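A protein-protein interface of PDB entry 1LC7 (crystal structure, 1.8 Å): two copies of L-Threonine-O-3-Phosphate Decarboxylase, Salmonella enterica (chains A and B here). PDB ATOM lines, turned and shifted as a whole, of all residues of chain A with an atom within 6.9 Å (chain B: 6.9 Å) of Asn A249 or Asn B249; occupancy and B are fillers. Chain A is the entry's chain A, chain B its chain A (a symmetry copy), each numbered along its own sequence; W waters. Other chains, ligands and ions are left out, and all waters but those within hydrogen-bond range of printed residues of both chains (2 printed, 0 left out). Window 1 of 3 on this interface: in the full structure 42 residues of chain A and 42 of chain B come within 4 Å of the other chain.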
ATOM      1  N   ILE A  53     -26.642  12.404  17.268  1.00  0.00           N
ATOM      2  CA  ILE A  53     -26.231  11.029  17.524  1.00  0.00           C
ATOM      3  C   ILE A  53     -25.809  10.286  16.247  1.00  0.00           C
ATOM      4  O   ILE A  53     -25.295   9.147  16.296  1.00  0.00           O
ATOM      5  CB  ILE A  53     -27.334  10.235  18.256  1.00  0.00           C
ATOM      6  CG1 ILE A  53     -28.588  10.151  17.378  1.00  0.00           C
ATOM      7  CG2 ILE A  53     -27.629  10.890  19.600  1.00  0.00           C
ATOM      8  CD1 ILE A  53     -29.634   9.194  17.911  1.00  0.00           C
ATOM      9  N   PRO A  57     -19.204  11.209  19.092  1.00  0.00           N
ATOM     10  CA  PRO A  57     -19.044  12.382  19.958  1.00  0.00           C
ATOM     11  C   PRO A  57     -17.624  12.872  19.648  1.00  0.00           C
ATOM     12  O   PRO A  57     -16.863  12.165  18.997  1.00  0.00           O
ATOM     13  CB  PRO A  57     -19.084  11.790  21.369  1.00  0.00           C
ATOM     14  CG  PRO A  57     -19.763  10.451  21.203  1.00  0.00           C
ATOM     15  CD  PRO A  57     -19.246   9.970  19.879  1.00  0.00           C
ATOM     16  N   TYR A  61     -13.995  15.827  23.694  1.00  0.00           N
ATOM     17  CA  TYR A  61     -15.067  16.563  24.380  1.00  0.00           C
ATOM     18  C   TYR A  61     -14.697  18.000  24.682  1.00  0.00           C
ATOM     19  O   TYR A  61     -14.821  18.466  25.818  1.00  0.00           O
ATOM     20  CB  TYR A  61     -15.482  15.848  25.670  1.00  0.00           C
ATOM     21  CG  TYR A  61     -15.949  14.442  25.376  1.00  0.00           C
ATOM     22  CD1 TYR A  61     -15.064  13.370  25.410  1.00  0.00           C
ATOM     23  CD2 TYR A  61     -17.252  14.217  24.952  1.00  0.00           C
ATOM     24  CE1 TYR A  61     -15.479  12.089  25.022  1.00  0.00           C
ATOM     25  CE2 TYR A  61     -17.689  12.944  24.555  1.00  0.00           C
ATOM     26  CZ  TYR A  61     -16.804  11.891  24.596  1.00  0.00           C
ATOM     27  OH  TYR A  61     -17.228  10.620  24.222  1.00  0.00           O
ATOM     28  N   LEU A  64     -17.784  20.166  26.151  1.00  0.00           N
ATOM     29  CA  LEU A  64     -18.113  19.722  27.511  1.00  0.00           C
ATOM     30  C   LEU A  64     -17.009  20.078  28.511  1.00  0.00           C
ATOM     31  O   LEU A  64     -17.291  20.611  29.592  1.00  0.00           O
ATOM     32  CB  LEU A  64     -18.349  18.198  27.539  1.00  0.00           C
ATOM     33  CG  LEU A  64     -18.540  17.583  28.947  1.00  0.00           C
ATOM     34  CD1 LEU A  64     -19.743  18.216  29.622  1.00  0.00           C
ATOM     35  CD2 LEU A  64     -18.704  16.069  28.844  1.00  0.00           C
ATOM     36  N   ASN A  83     -18.218   8.274  31.603  1.00  0.00           N
ATOM     37  CA  ASN A  83     -19.544   7.665  31.389  1.00  0.00           C
ATOM     38  C   ASN A  83     -20.127   7.332  32.751  1.00  0.00           C
ATOM     39  O   ASN A  83     -20.263   6.163  33.128  1.00  0.00           O
ATOM     40  CB  ASN A  83     -19.324   6.390  30.551  1.00  0.00           C
ATOM     41  CG  ASN A  83     -20.597   5.733  30.153  1.00  0.00           C
ATOM     42  OD1 ASN A  83     -21.545   6.403  29.768  1.00  0.00           O
ATOM     43  ND2 ASN A  83     -20.628   4.411  30.210  1.00  0.00           N
ATOM     44  N   PRO A 221     -29.561  10.344  35.470  1.00  0.00           N
ATOM     45  CA  PRO A 221     -28.793   9.115  35.644  1.00  0.00           C
ATOM     46  C   PRO A 221     -28.802   8.204  34.437  1.00  0.00           C
ATOM     47  O   PRO A 221     -27.892   7.390  34.266  1.00  0.00           O
ATOM     48  CB  PRO A 221     -29.444   8.475  36.863  1.00  0.00           C
ATOM     49  CG  PRO A 221     -30.846   8.934  36.780  1.00  0.00           C
ATOM     50  CD  PRO A 221     -30.684  10.400  36.421  1.00  0.00           C
ATOM     51  N   GLY A 222     -29.845   8.322  33.613  1.00  0.00           N
ATOM     52  CA  GLY A 222     -29.934   7.474  32.433  1.00  0.00           C
ATOM     53  C   GLY A 222     -29.001   7.880  31.312  1.00  0.00           C
ATOM     54  O   GLY A 222     -28.752   7.089  30.399  1.00  0.00           O
ATOM     55  N   LEU A 223     -28.504   9.113  31.355  1.00  0.00           N
ATOM     56  CA  LEU A 223     -27.568   9.617  30.339  1.00  0.00           C
ATOM     57  C   LEU A 223     -26.117   9.223  30.633  1.00  0.00           C
ATOM     58  O   LEU A 223     -25.321   9.045  29.709  1.00  0.00           O
ATOM     59  CB  LEU A 223     -27.672  11.141  30.231  1.00  0.00           C
ATOM     60  CG  LEU A 223     -28.768  11.628  29.251  1.00  0.00           C
ATOM     61  CD1 LEU A 223     -28.669  13.136  29.088  1.00  0.00           C
ATOM     62  CD2 LEU A 223     -28.583  10.966  27.907  1.00  0.00           C
ATOM     63  N   ARG A 224     -25.801   9.068  31.913  1.00  0.00           N
ATOM     64  CA  ARG A 224     -24.460   8.671  32.387  1.00  0.00           C
ATOM     65  C   ARG A 224     -23.420   9.784  32.216  1.00  0.00           C
ATOM     66  O   ARG A 224     -22.870   9.963  31.140  1.00  0.00           O
ATOM     67  CB  ARG A 224     -23.980   7.412  31.660  1.00  0.00           C
ATOM     68  CG  ARG A 224     -24.984   6.227  31.575  1.00  0.00           C
ATOM     69  CD  ARG A 224     -25.487   5.709  32.900  1.00  0.00           C
ATOM     70  NE  ARG A 224     -24.409   5.265  33.763  1.00  0.00           N
ATOM     71  CZ  ARG A 224     -24.174   5.791  34.961  1.00  0.00           C
ATOM     72  NH1 ARG A 224     -24.945   6.756  35.418  1.00  0.00           N
ATOM     73  NH2 ARG A 224     -23.159   5.370  35.701  1.00  0.00           N
ATOM     74  N   LEU A 225     -23.154  10.550  33.264  1.00  0.00           N
ATOM     75  CA  LEU A 225     -22.149  11.595  33.128  1.00  0.00           C
ATOM     76  C   LEU A 225     -21.528  11.996  34.444  1.00  0.00           C
ATOM     77  O   LEU A 225     -22.231  12.346  35.396  1.00  0.00           O
ATOM     78  CB  LEU A 225     -22.760  12.836  32.463  1.00  0.00           C
ATOM     79  CG  LEU A 225     -21.817  14.002  32.211  1.00  0.00           C
ATOM     80  CD1 LEU A 225     -20.727  13.573  31.237  1.00  0.00           C
ATOM     81  CD2 LEU A 225     -22.611  15.200  31.614  1.00  0.00           C
ATOM     82  N   TRP A 246     -14.360   7.764  23.188  1.00  0.00           N
ATOM     83  CA  TRP A 246     -15.782   8.079  23.086  1.00  0.00           C
ATOM     84  C   TRP A 246     -16.623   7.491  24.189  1.00  0.00           C
ATOM     85  O   TRP A 246     -17.717   6.992  23.932  1.00  0.00           O
ATOM     86  CB  TRP A 246     -16.343   7.545  21.765  1.00  0.00           C
ATOM     87  CG  TRP A 246     -15.562   7.901  20.536  1.00  0.00           C
ATOM     88  CD1 TRP A 246     -15.409   9.144  19.977  1.00  0.00           C
ATOM     89  CD2 TRP A 246     -14.979   6.965  19.621  1.00  0.00           C
ATOM     90  NE1 TRP A 246     -14.778   9.028  18.739  1.00  0.00           N
ATOM     91  CE2 TRP A 246     -14.504   7.703  18.508  1.00  0.00           C
ATOM     92  CE3 TRP A 246     -14.823   5.568  19.631  1.00  0.00           C
ATOM     93  CZ2 TRP A 246     -13.881   7.088  17.417  1.00  0.00           C
ATOM     94  CZ3 TRP A 246     -14.202   4.950  18.543  1.00  0.00           C
ATOM     95  CH2 TRP A 246     -13.739   5.719  17.447  1.00  0.00           C
ATOM     96  N   SER A 247     -16.113   7.515  25.412  1.00  0.00           N
ATOM     97  CA  SER A 247     -16.837   6.990  26.569  1.00  0.00           C
ATOM     98  C   SER A 247     -18.154   7.711  26.846  1.00  0.00           C
ATOM     99  O   SER A 247     -19.123   7.077  27.280  1.00  0.00           O
ATOM    100  CB  SER A 247     -15.966   7.140  27.852  1.00  0.00           C
ATOM    101  OG  SER A 247     -14.926   6.220  27.867  1.00  0.00           O
ATOM    102  N   VAL A 248     -18.176   9.022  26.614  1.00  0.00           N
ATOM    103  CA  VAL A 248     -19.359   9.851  26.904  1.00  0.00           C
ATOM    104  C   VAL A 248     -20.226   9.956  25.658  1.00  0.00           C
ATOM    105  O   VAL A 248     -19.720  10.311  24.586  1.00  0.00           O
ATOM    106  CB  VAL A 248     -18.893  11.278  27.406  1.00  0.00           C
ATOM    107  CG1 VAL A 248     -20.107  12.212  27.615  1.00  0.00           C
ATOM    108  CG2 VAL A 248     -18.120  11.117  28.724  1.00  0.00           C
ATOM    109  N   ASN A 249     -21.511   9.616  25.769  1.00  0.00           N
ATOM    110  CA  ASN A 249     -22.345   9.691  24.587  1.00  0.00           C
ATOM    111  C   ASN A 249     -22.653  11.145  24.280  1.00  0.00           C
ATOM    112  O   ASN A 249     -22.574  12.025  25.155  1.00  0.00           O
ATOM    113  CB  ASN A 249     -23.608   8.815  24.719  1.00  0.00           C
ATOM    114  CG  ASN A 249     -24.565   9.311  25.752  1.00  0.00           C
ATOM    115  OD1 ASN A 249     -25.345  10.249  25.500  1.00  0.00           O
ATOM    116  ND2 ASN A 249     -24.522   8.694  26.936  1.00  0.00           N
ATOM    117  N   ALA A 250     -22.959  11.410  23.016  1.00  0.00           N
ATOM    118  CA  ALA A 250     -23.203  12.779  22.560  1.00  0.00           C
ATOM    119  C   ALA A 250     -24.306  13.536  23.297  1.00  0.00           C
ATOM    120  O   ALA A 250     -24.168  14.738  23.539  1.00  0.00           O
ATOM    121  CB  ALA A 250     -23.495  12.770  21.059  1.00  0.00           C
ATOM    122  N   LEU A 251     -25.382  12.850  23.669  1.00  0.00           N
ATOM    123  CA  LEU A 251     -26.477  13.526  24.380  1.00  0.00           C
ATOM    124  C   LEU A 251     -26.085  13.841  25.805  1.00  0.00           C
ATOM    125  O   LEU A 251     -26.478  14.885  26.346  1.00  0.00           O
ATOM    126  CB  LEU A 251     -27.747  12.679  24.340  1.00  0.00           C
ATOM    127  CG  LEU A 251     -28.198  12.341  22.913  1.00  0.00           C
ATOM    128  CD1 LEU A 251     -29.489  11.542  22.939  1.00  0.00           C
ATOM    129  CD2 LEU A 251     -28.358  13.640  22.125  1.00  0.00           C
ATOM    130  N   ALA A 252     -25.282  12.972  26.423  1.00  0.00           N
ATOM    131  CA  ALA A 252     -24.852  13.272  27.771  1.00  0.00           C
ATOM    132  C   ALA A 252     -23.964  14.503  27.736  1.00  0.00           C
ATOM    133  O   ALA A 252     -24.048  15.339  28.627  1.00  0.00           O
ATOM    134  CB  ALA A 252     -24.098  12.062  28.378  1.00  0.00           C
ATOM    135  N   ALA A 253     -23.118  14.625  26.714  1.00  0.00           N
ATOM    136  CA  ALA A 253     -22.224  15.776  26.637  1.00  0.00           C
ATOM    137  C   ALA A 253     -23.041  17.070  26.501  1.00  0.00           C
ATOM    138  O   ALA A 253     -22.741  18.071  27.142  1.00  0.00           O
ATOM    139  CB  ALA A 253     -21.241  15.627  25.479  1.00  0.00           C
ATOM    140  N   LEU A 254     -24.084  17.005  25.683  1.00  0.00           N
ATOM    141  CA  LEU A 254     -24.985  18.125  25.439  1.00  0.00           C
ATOM    142  C   LEU A 254     -25.760  18.492  26.701  1.00  0.00           C
ATOM    143  O   LEU A 254     -25.812  19.662  27.091  1.00  0.00           O
ATOM    144  CB  LEU A 254     -25.956  17.754  24.329  1.00  0.00           C
ATOM    145  CG  LEU A 254     -27.174  18.660  24.182  1.00  0.00           C
ATOM    146  CD1 LEU A 254     -26.760  19.980  23.552  1.00  0.00           C
ATOM    147  CD2 LEU A 254     -28.203  17.947  23.312  1.00  0.00           C
ATOM    148  N   ILE B  53     -34.461   9.051  30.968  1.00  0.00           N
ATOM    149  CA  ILE B  53     -33.120   9.356  31.451  1.00  0.00           C
ATOM    150  C   ILE B  53     -33.105   9.832  32.911  1.00  0.00           C
ATOM    151  O   ILE B  53     -32.032  10.002  33.531  1.00  0.00           O
ATOM    152  CB  ILE B  53     -32.415  10.394  30.551  1.00  0.00           C
ATOM    153  CG1 ILE B  53     -33.190  11.717  30.574  1.00  0.00           C
ATOM    154  CG2 ILE B  53     -32.287   9.841  29.136  1.00  0.00           C
ATOM    155  CD1 ILE B  53     -32.449  12.860  29.913  1.00  0.00           C
ATOM    156  N   PRO B  57     -30.375   3.204  33.999  1.00  0.00           N
ATOM    157  CA  PRO B  57     -30.783   2.183  33.028  1.00  0.00           C
ATOM    158  C   PRO B  57     -30.925   0.912  33.876  1.00  0.00           C
ATOM    159  O   PRO B  57     -30.502   0.895  35.026  1.00  0.00           O
ATOM    160  CB  PRO B  57     -29.561   2.052  32.115  1.00  0.00           C
ATOM    161  CG  PRO B  57     -28.792   3.337  32.318  1.00  0.00           C
ATOM    162  CD  PRO B  57     -28.983   3.619  33.780  1.00  0.00           C
ATOM    163  N   TYR B  61     -30.006  -4.823  31.746  1.00  0.00           N
ATOM    164  CA  TYR B  61     -30.524  -4.587  30.390  1.00  0.00           C
ATOM    165  C   TYR B  61     -31.385  -5.724  29.881  1.00  0.00           C
ATOM    166  O   TYR B  61     -31.171  -6.245  28.783  1.00  0.00           O
ATOM    167  CB  TYR B  61     -29.380  -4.318  29.407  1.00  0.00           C
ATOM    168  CG  TYR B  61     -28.567  -3.123  29.847  1.00  0.00           C
ATOM    169  CD1 TYR B  61     -27.447  -3.276  30.658  1.00  0.00           C
ATOM    170  CD2 TYR B  61     -28.997  -1.839  29.541  1.00  0.00           C
ATOM    171  CE1 TYR B  61     -26.768  -2.156  31.156  1.00  0.00           C
ATOM    172  CE2 TYR B  61     -28.336  -0.703  30.033  1.00  0.00           C
ATOM    173  CZ  TYR B  61     -27.228  -0.868  30.832  1.00  0.00           C
ATOM    174  OH  TYR B  61     -26.552   0.249  31.311  1.00  0.00           O
ATOM    175  N   LEU B  64     -33.188  -4.901  26.353  1.00  0.00           N
ATOM    176  CA  LEU B  64     -32.194  -4.863  25.272  1.00  0.00           C
ATOM    177  C   LEU B  64     -31.612  -6.250  24.983  1.00  0.00           C
ATOM    178  O   LEU B  64     -31.527  -6.663  23.819  1.00  0.00           O
ATOM    179  CB  LEU B  64     -31.047  -3.897  25.628  1.00  0.00           C
ATOM    180  CG  LEU B  64     -29.853  -3.895  24.643  1.00  0.00           C
ATOM    181  CD1 LEU B  64     -30.333  -3.499  23.259  1.00  0.00           C
ATOM    182  CD2 LEU B  64     -28.763  -2.947  25.137  1.00  0.00           C
ATOM    183  N   ASN B  83     -20.980  -0.205  25.860  1.00  0.00           N
ATOM    184  CA  ASN B  83     -21.001   1.227  25.507  1.00  0.00           C
ATOM    185  C   ASN B  83     -20.167   1.407  24.250  1.00  0.00           C
ATOM    186  O   ASN B  83     -19.081   1.995  24.274  1.00  0.00           O
ATOM    187  CB  ASN B  83     -20.387   1.993  26.696  1.00  0.00           C
ATOM    188  CG  ASN B  83     -20.454   3.469  26.529  1.00  0.00           C
ATOM    189  OD1 ASN B  83     -21.466   3.997  26.088  1.00  0.00           O
ATOM    190  ND2 ASN B  83     -19.390   4.160  26.907  1.00  0.00           N
ATOM    191  N   PRO B 221     -23.795   6.378  16.029  1.00  0.00           N
ATOM    192  CA  PRO B 221     -22.510   6.352  16.720  1.00  0.00           C
ATOM    193  C   PRO B 221     -22.451   7.232  17.948  1.00  0.00           C
ATOM    194  O   PRO B 221     -21.638   6.994  18.845  1.00  0.00           O
ATOM    195  CB  PRO B 221     -21.532   6.792  15.639  1.00  0.00           C
ATOM    196  CG  PRO B 221     -22.345   7.687  14.789  1.00  0.00           C
ATOM    197  CD  PRO B 221     -23.648   6.918  14.667  1.00  0.00           C
ATOM    198  N   GLY B 222     -23.294   8.267  17.978  1.00  0.00           N
ATOM    199  CA  GLY B 222     -23.292   9.168  19.122  1.00  0.00           C
ATOM    200  C   GLY B 222     -23.950   8.594  20.358  1.00  0.00           C
ATOM    201  O   GLY B 222     -23.751   9.111  21.459  1.00  0.00           O
ATOM    202  N   LEU B 223     -24.755   7.549  20.185  1.00  0.00           N
ATOM    203  CA  LEU B 223     -25.433   6.887  21.310  1.00  0.00           C
ATOM    204  C   LEU B 223     -24.542   5.851  22.002  1.00  0.00           C
ATOM    205  O   LEU B 223     -24.673   5.622  23.207  1.00  0.00           O
ATOM    206  CB  LEU B 223     -26.723   6.215  20.830  1.00  0.00           C
ATOM    207  CG  LEU B 223     -27.956   7.151  20.830  1.00  0.00           C
ATOM    208  CD1 LEU B 223     -29.205   6.346  20.508  1.00  0.00           C
ATOM    209  CD2 LEU B 223     -28.111   7.796  22.186  1.00  0.00           C
ATOM    210  N   ARG B 224     -23.633   5.257  21.238  1.00  0.00           N
ATOM    211  CA  ARG B 224     -22.674   4.249  21.733  1.00  0.00           C
ATOM    212  C   ARG B 224     -23.343   2.909  22.060  1.00  0.00           C
ATOM    213  O   ARG B 224     -23.910   2.740  23.130  1.00  0.00           O
ATOM    214  CB  ARG B 224     -21.938   4.765  22.972  1.00  0.00           C
ATOM    215  CG  ARG B 224     -21.342   6.198  22.886  1.00  0.00           C
ATOM    216  CD  ARG B 224     -20.359   6.423  21.762  1.00  0.00           C
ATOM    217  NE  ARG B 224     -19.229   5.517  21.830  1.00  0.00           N
ATOM    218  CZ  ARG B 224     -18.924   4.662  20.859  1.00  0.00           C
ATOM    219  NH1 ARG B 224     -19.660   4.617  19.767  1.00  0.00           N
ATOM    220  NH2 ARG B 224     -17.897   3.834  20.980  1.00  0.00           N
ATOM    221  N   LEU B 225     -23.301   1.954  21.142  1.00  0.00           N
ATOM    222  CA  LEU B 225     -23.907   0.666  21.446  1.00  0.00           C
ATOM    223  C   LEU B 225     -23.329  -0.468  20.635  1.00  0.00           C
ATOM    224  O   LEU B 225     -23.291  -0.413  19.403  1.00  0.00           O
ATOM    225  CB  LEU B 225     -25.423   0.724  21.215  1.00  0.00           C
ATOM    226  CG  LEU B 225     -26.206  -0.540  21.535  1.00  0.00           C
ATOM    227  CD1 LEU B 225     -26.082  -0.853  23.020  1.00  0.00           C
ATOM    228  CD2 LEU B 225     -27.705  -0.337  21.166  1.00  0.00           C
ATOM    229  N   TRP B 246     -24.033  -0.187  34.614  1.00  0.00           N
ATOM    230  CA  TRP B 246     -24.748   0.804  33.816  1.00  0.00           C
ATOM    231  C   TRP B 246     -23.928   1.405  32.704  1.00  0.00           C
ATOM    232  O   TRP B 246     -23.992   2.612  32.473  1.00  0.00           O
ATOM    233  CB  TRP B 246     -25.207   1.962  34.708  1.00  0.00           C
ATOM    234  CG  TRP B 246     -25.929   1.570  35.961  1.00  0.00           C
ATOM    235  CD1 TRP B 246     -27.167   0.990  36.063  1.00  0.00           C
ATOM    236  CD2 TRP B 246     -25.519   1.899  37.295  1.00  0.00           C
ATOM    237  NE1 TRP B 246     -27.566   0.964  37.399  1.00  0.00           N
ATOM    238  CE2 TRP B 246     -26.568   1.512  38.166  1.00  0.00           C
ATOM    239  CE3 TRP B 246     -24.368   2.497  37.835  1.00  0.00           C
ATOM    240  CZ2 TRP B 246     -26.495   1.702  39.549  1.00  0.00           C
ATOM    241  CZ3 TRP B 246     -24.292   2.689  39.217  1.00  0.00           C
ATOM    242  CH2 TRP B 246     -25.359   2.289  40.058  1.00  0.00           C
ATOM    243  N   SER B 247     -23.135   0.586  32.030  1.00  0.00           N
ATOM    244  CA  SER B 247     -22.303   1.044  30.919  1.00  0.00           C
ATOM    245  C   SER B 247     -23.102   1.617  29.750  1.00  0.00           C
ATOM    246  O   SER B 247     -22.647   2.564  29.100  1.00  0.00           O
ATOM    247  CB  SER B 247     -21.472  -0.146  30.353  1.00  0.00           C
ATOM    248  OG  SER B 247     -20.438  -0.494  31.212  1.00  0.00           O
ATOM    249  N   VAL B 248     -24.267   1.031  29.482  1.00  0.00           N
ATOM    250  CA  VAL B 248     -25.106   1.437  28.341  1.00  0.00           C
ATOM    251  C   VAL B 248     -26.117   2.479  28.795  1.00  0.00           C
ATOM    252  O   VAL B 248     -26.833   2.253  29.779  1.00  0.00           O
ATOM    253  CB  VAL B 248     -25.823   0.163  27.733  1.00  0.00           C
ATOM    254  CG1 VAL B 248     -26.797   0.567  26.602  1.00  0.00           C
ATOM    255  CG2 VAL B 248     -24.757  -0.800  27.190  1.00  0.00           C
ATOM    256  N   ASN B 249     -26.160   3.631  28.125  1.00  0.00           N
ATOM    257  CA  ASN B 249     -27.103   4.642  28.558  1.00  0.00           C
ATOM    258  C   ASN B 249     -28.505   4.233  28.145  1.00  0.00           C
ATOM    259  O   ASN B 249     -28.701   3.424  27.222  1.00  0.00           O
ATOM    260  CB  ASN B 249     -26.706   6.048  28.062  1.00  0.00           C
ATOM    261  CG  ASN B 249     -26.814   6.202  26.580  1.00  0.00           C
ATOM    262  OD1 ASN B 249     -27.916   6.415  26.040  1.00  0.00           O
ATOM    263  ND2 ASN B 249     -25.672   6.095  25.896  1.00  0.00           N
ATOM    264  N   ALA B 250     -29.489   4.757  28.866  1.00  0.00           N
ATOM    265  CA  ALA B 250     -30.886   4.391  28.630  1.00  0.00           C
ATOM    266  C   ALA B 250     -31.402   4.623  27.212  1.00  0.00           C
ATOM    267  O   ALA B 250     -32.178   3.810  26.701  1.00  0.00           O
ATOM    268  CB  ALA B 250     -31.779   5.124  29.633  1.00  0.00           C
ATOM    269  N   LEU B 251     -30.971   5.703  26.569  1.00  0.00           N
ATOM    270  CA  LEU B 251     -31.434   5.980  25.200  1.00  0.00           C
ATOM    271  C   LEU B 251     -30.796   5.034  24.210  1.00  0.00           C
ATOM    272  O   LEU B 251     -31.437   4.623  23.233  1.00  0.00           O
ATOM    273  CB  LEU B 251     -31.156   7.432  24.823  1.00  0.00           C
ATOM    274  CG  LEU B 251     -31.796   8.437  25.790  1.00  0.00           C
ATOM    275  CD1 LEU B 251     -31.526   9.860  25.334  1.00  0.00           C
ATOM    276  CD2 LEU B 251     -33.294   8.151  25.879  1.00  0.00           C
ATOM    277  N   ALA B 252     -29.542   4.647  24.458  1.00  0.00           N
ATOM    278  CA  ALA B 252     -28.921   3.705  23.552  1.00  0.00           C
ATOM    279  C   ALA B 252     -29.654   2.378  23.653  1.00  0.00           C
ATOM    280  O   ALA B 252     -29.853   1.716  22.643  1.00  0.00           O
ATOM    281  CB  ALA B 252     -27.420   3.536  23.895  1.00  0.00           C
ATOM    282  N   ALA B 253     -30.061   1.988  24.860  1.00  0.00           N
ATOM    283  CA  ALA B 253     -30.750   0.712  25.024  1.00  0.00           C
ATOM    284  C   ALA B 253     -32.080   0.730  24.255  1.00  0.00           C
ATOM    285  O   ALA B 253     -32.434  -0.238  23.591  1.00  0.00           O
ATOM    286  CB  ALA B 253     -30.977   0.398  26.500  1.00  0.00           C
ATOM    287  N   LEU B 254     -32.776   1.858  24.341  1.00  0.00           N
ATOM    288  CA  LEU B 254     -34.052   2.068  23.668  1.00  0.00           C
ATOM    289  C   LEU B 254     -33.880   2.069  22.152  1.00  0.00           C
ATOM    290  O   LEU B 254     -34.605   1.375  21.434  1.00  0.00           O
ATOM    291  CB  LEU B 254     -34.643   3.394  24.120  1.00  0.00           C
ATOM    292  CG  LEU B 254     -35.790   3.933  23.270  1.00  0.00           C
ATOM    293  CD1 LEU B 254     -37.052   3.131  23.543  1.00  0.00           C
ATOM    294  CD2 LEU B 254     -35.998   5.402  23.619  1.00  0.00           C
HETATM  295  O   HOH W   1     -17.041   4.021  23.607  1.00  0.00           O
HETATM  296  O   HOH W   2     -21.631   3.727  34.077  1.00  0.00           O
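The backbone carbonyl oxygen (O) of Ile A53 lies within hydrogen-bond range of the backbone NH (N) of Gly B222 (2.8 Å). The side-chain amide nitrogen (ND2) of Asn A83 sits at hydrogen-bond distance from the backbone carbonyl oxygen (O) of Ser B247 (3.0 Å). N of Gly A222 is in hydrogen-bond range of O of Ile B53 (2.8 Å). N of Ala B250 lies within hydrogen-bond range of O of Gly A222 (2.9 Å). NE of Arg A224 is in hydrogen-bond range of O of Trp B246 (3.0 Å). O of Trp A246 sits at hydrogen-bond distance from NE of Arg B224 (3.0 Å). The side-chain amide nitrogen (ND2) of Asn B83 sits at hydrogen-bond distance from the backbone carbonyl oxygen (O) of Ser A247, 3.0 Å away. ND2 of Asn B249 sits close to ND2 of Asn A249, 3.0 Å away. The backbone NH of Ala A250 lies within hydrogen-bond range of the backbone carbonyl oxygen of Gly B222. O of Ile A53 lies close to N of Pro B221, at 3.2 Å. N of Pro A221 sits close to O of Ile B53 (3.2 Å).
NH1 of Arg A224 sits at hydrogen-bond distance from O of Pro A221, 3.2 Å away. OD1 of Asn A249 lies within hydrogen-bond range of N of Leu A251, at 3.2 Å. The backbone NH of Ala A252 lies within hydrogen-bond range of the side-chain amide oxygen of Asn A249, at 2.9 Å. NH1 of Arg B224 is in hydrogen-bond range of O of Pro B221 (3.2 Å). The backbone NH of Ala B252 sits at hydrogen-bond distance from the side-chain amide oxygen of Asn B249, at 2.9 Å.
Among the printed residues, merely in contact across the chains: Gly A222 with Asn B249 (3.3 Å), Asn A249 with Gly B222 (3.3 Å), Asn A83 with Asn B83 (3.5 Å), Leu A251 with Leu B251 (3.6 Å), Leu A223 with Asn B249 (3.7 Å), Asn A249 with Leu B223 (3.7 Å), Ile A53 with Leu B223 (3.9 Å), Leu A223 with Ile B53 (3.9 Å), Arg A224 with Asn B249 (3.9 Å), Asn A249 with Arg B224 (3.9 Å), Pro A221 with Pro B57 (3.96 Å) and Pro A57 with Pro B221 (3.96 Å).
Of chain B, only Gly B222 (3.3 Å), Leu B223 (3.7 Å), Arg B224 (3.9 Å) and Asn B249 (3.0 Å) come within 4 Å of Asn A249. Of chain A, only Gly A222 (3.3 Å), Leu A223 (3.7 Å), Arg A224 (3.9 Å) and Asn A249 (3.0 Å) come within 4 Å of Asn B249. Printed residues of chain A within 4 Å of Arg B224: Trp A246 (3.0 Å) and Asn A249 (3.9 Å). Of the printed residues of chain B, Arg A224 touches Trp B246 and Asn B249. Of the printed residues of chain B, Asn A83 touches Asn B83 (3.5 Å) and Ser B247 (3.0 Å). Printed residues of chain B within 4 Å of Trp A246: Arg B224 (3.0 Å). The nearest printed residue of chain A that does not touch Ser B247 is Arg A224 (5.0 Å).
Of the 19 printed residues of chain B, 12 touch a printed residue of chain A. Printed residues of chain B that touch a printed residue of chain A: Ile B53, Pro B57, Asn B83, Pro B221, Gly B222, Leu B223, Arg B224, Trp B246, Ser B247, Asn B249, Ala B250 and Leu B251. Hydrophobic or aromatic side chains of chain B that line the printed part of chain A: Ile B53, Pro B57, Pro B221, Leu B223, Trp B246, Ala B250 and Leu B251. Hydrophobic or aromatic side chains of chain A within 4 Å of the printed part of chain B: Ile A53, Pro A57, Pro A221, Leu A223, Trp A246, Ala A250 and Leu A251. Among the printed residues, no Asp or Glu carboxylate lies within 4 Å of a Lys or Arg side-chain nitrogen of the other chain.
Ile A53 touches Pro B221, and with the chains exchanged Pro A221 touches Ile B53. Ile A53 touches Gly B222, and with the chains exchanged Gly A222 touches Ile B53. Pro A57 touches Pro B221, and with the chains exchanged Pro A221 touches Pro B57. Arg A224 touches Asn B249, and with the chains exchanged Asn A249 touches Arg B224. 19 positions are printed for both chains.
Water W2 lies within hydrogen-bond range of NH2 of Arg A224 (2.8 Å), O of Asn A83 (3.0 Å) and O of Trp B246 (3.1 Å). Water W1 lies within hydrogen-bond range of the guanidinium group of Arg B224 (2.8 Å), the backbone carbonyl oxygen of Asn B83 (3.0 Å) and the backbone carbonyl oxygen of Trp A246 (3.1 Å).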
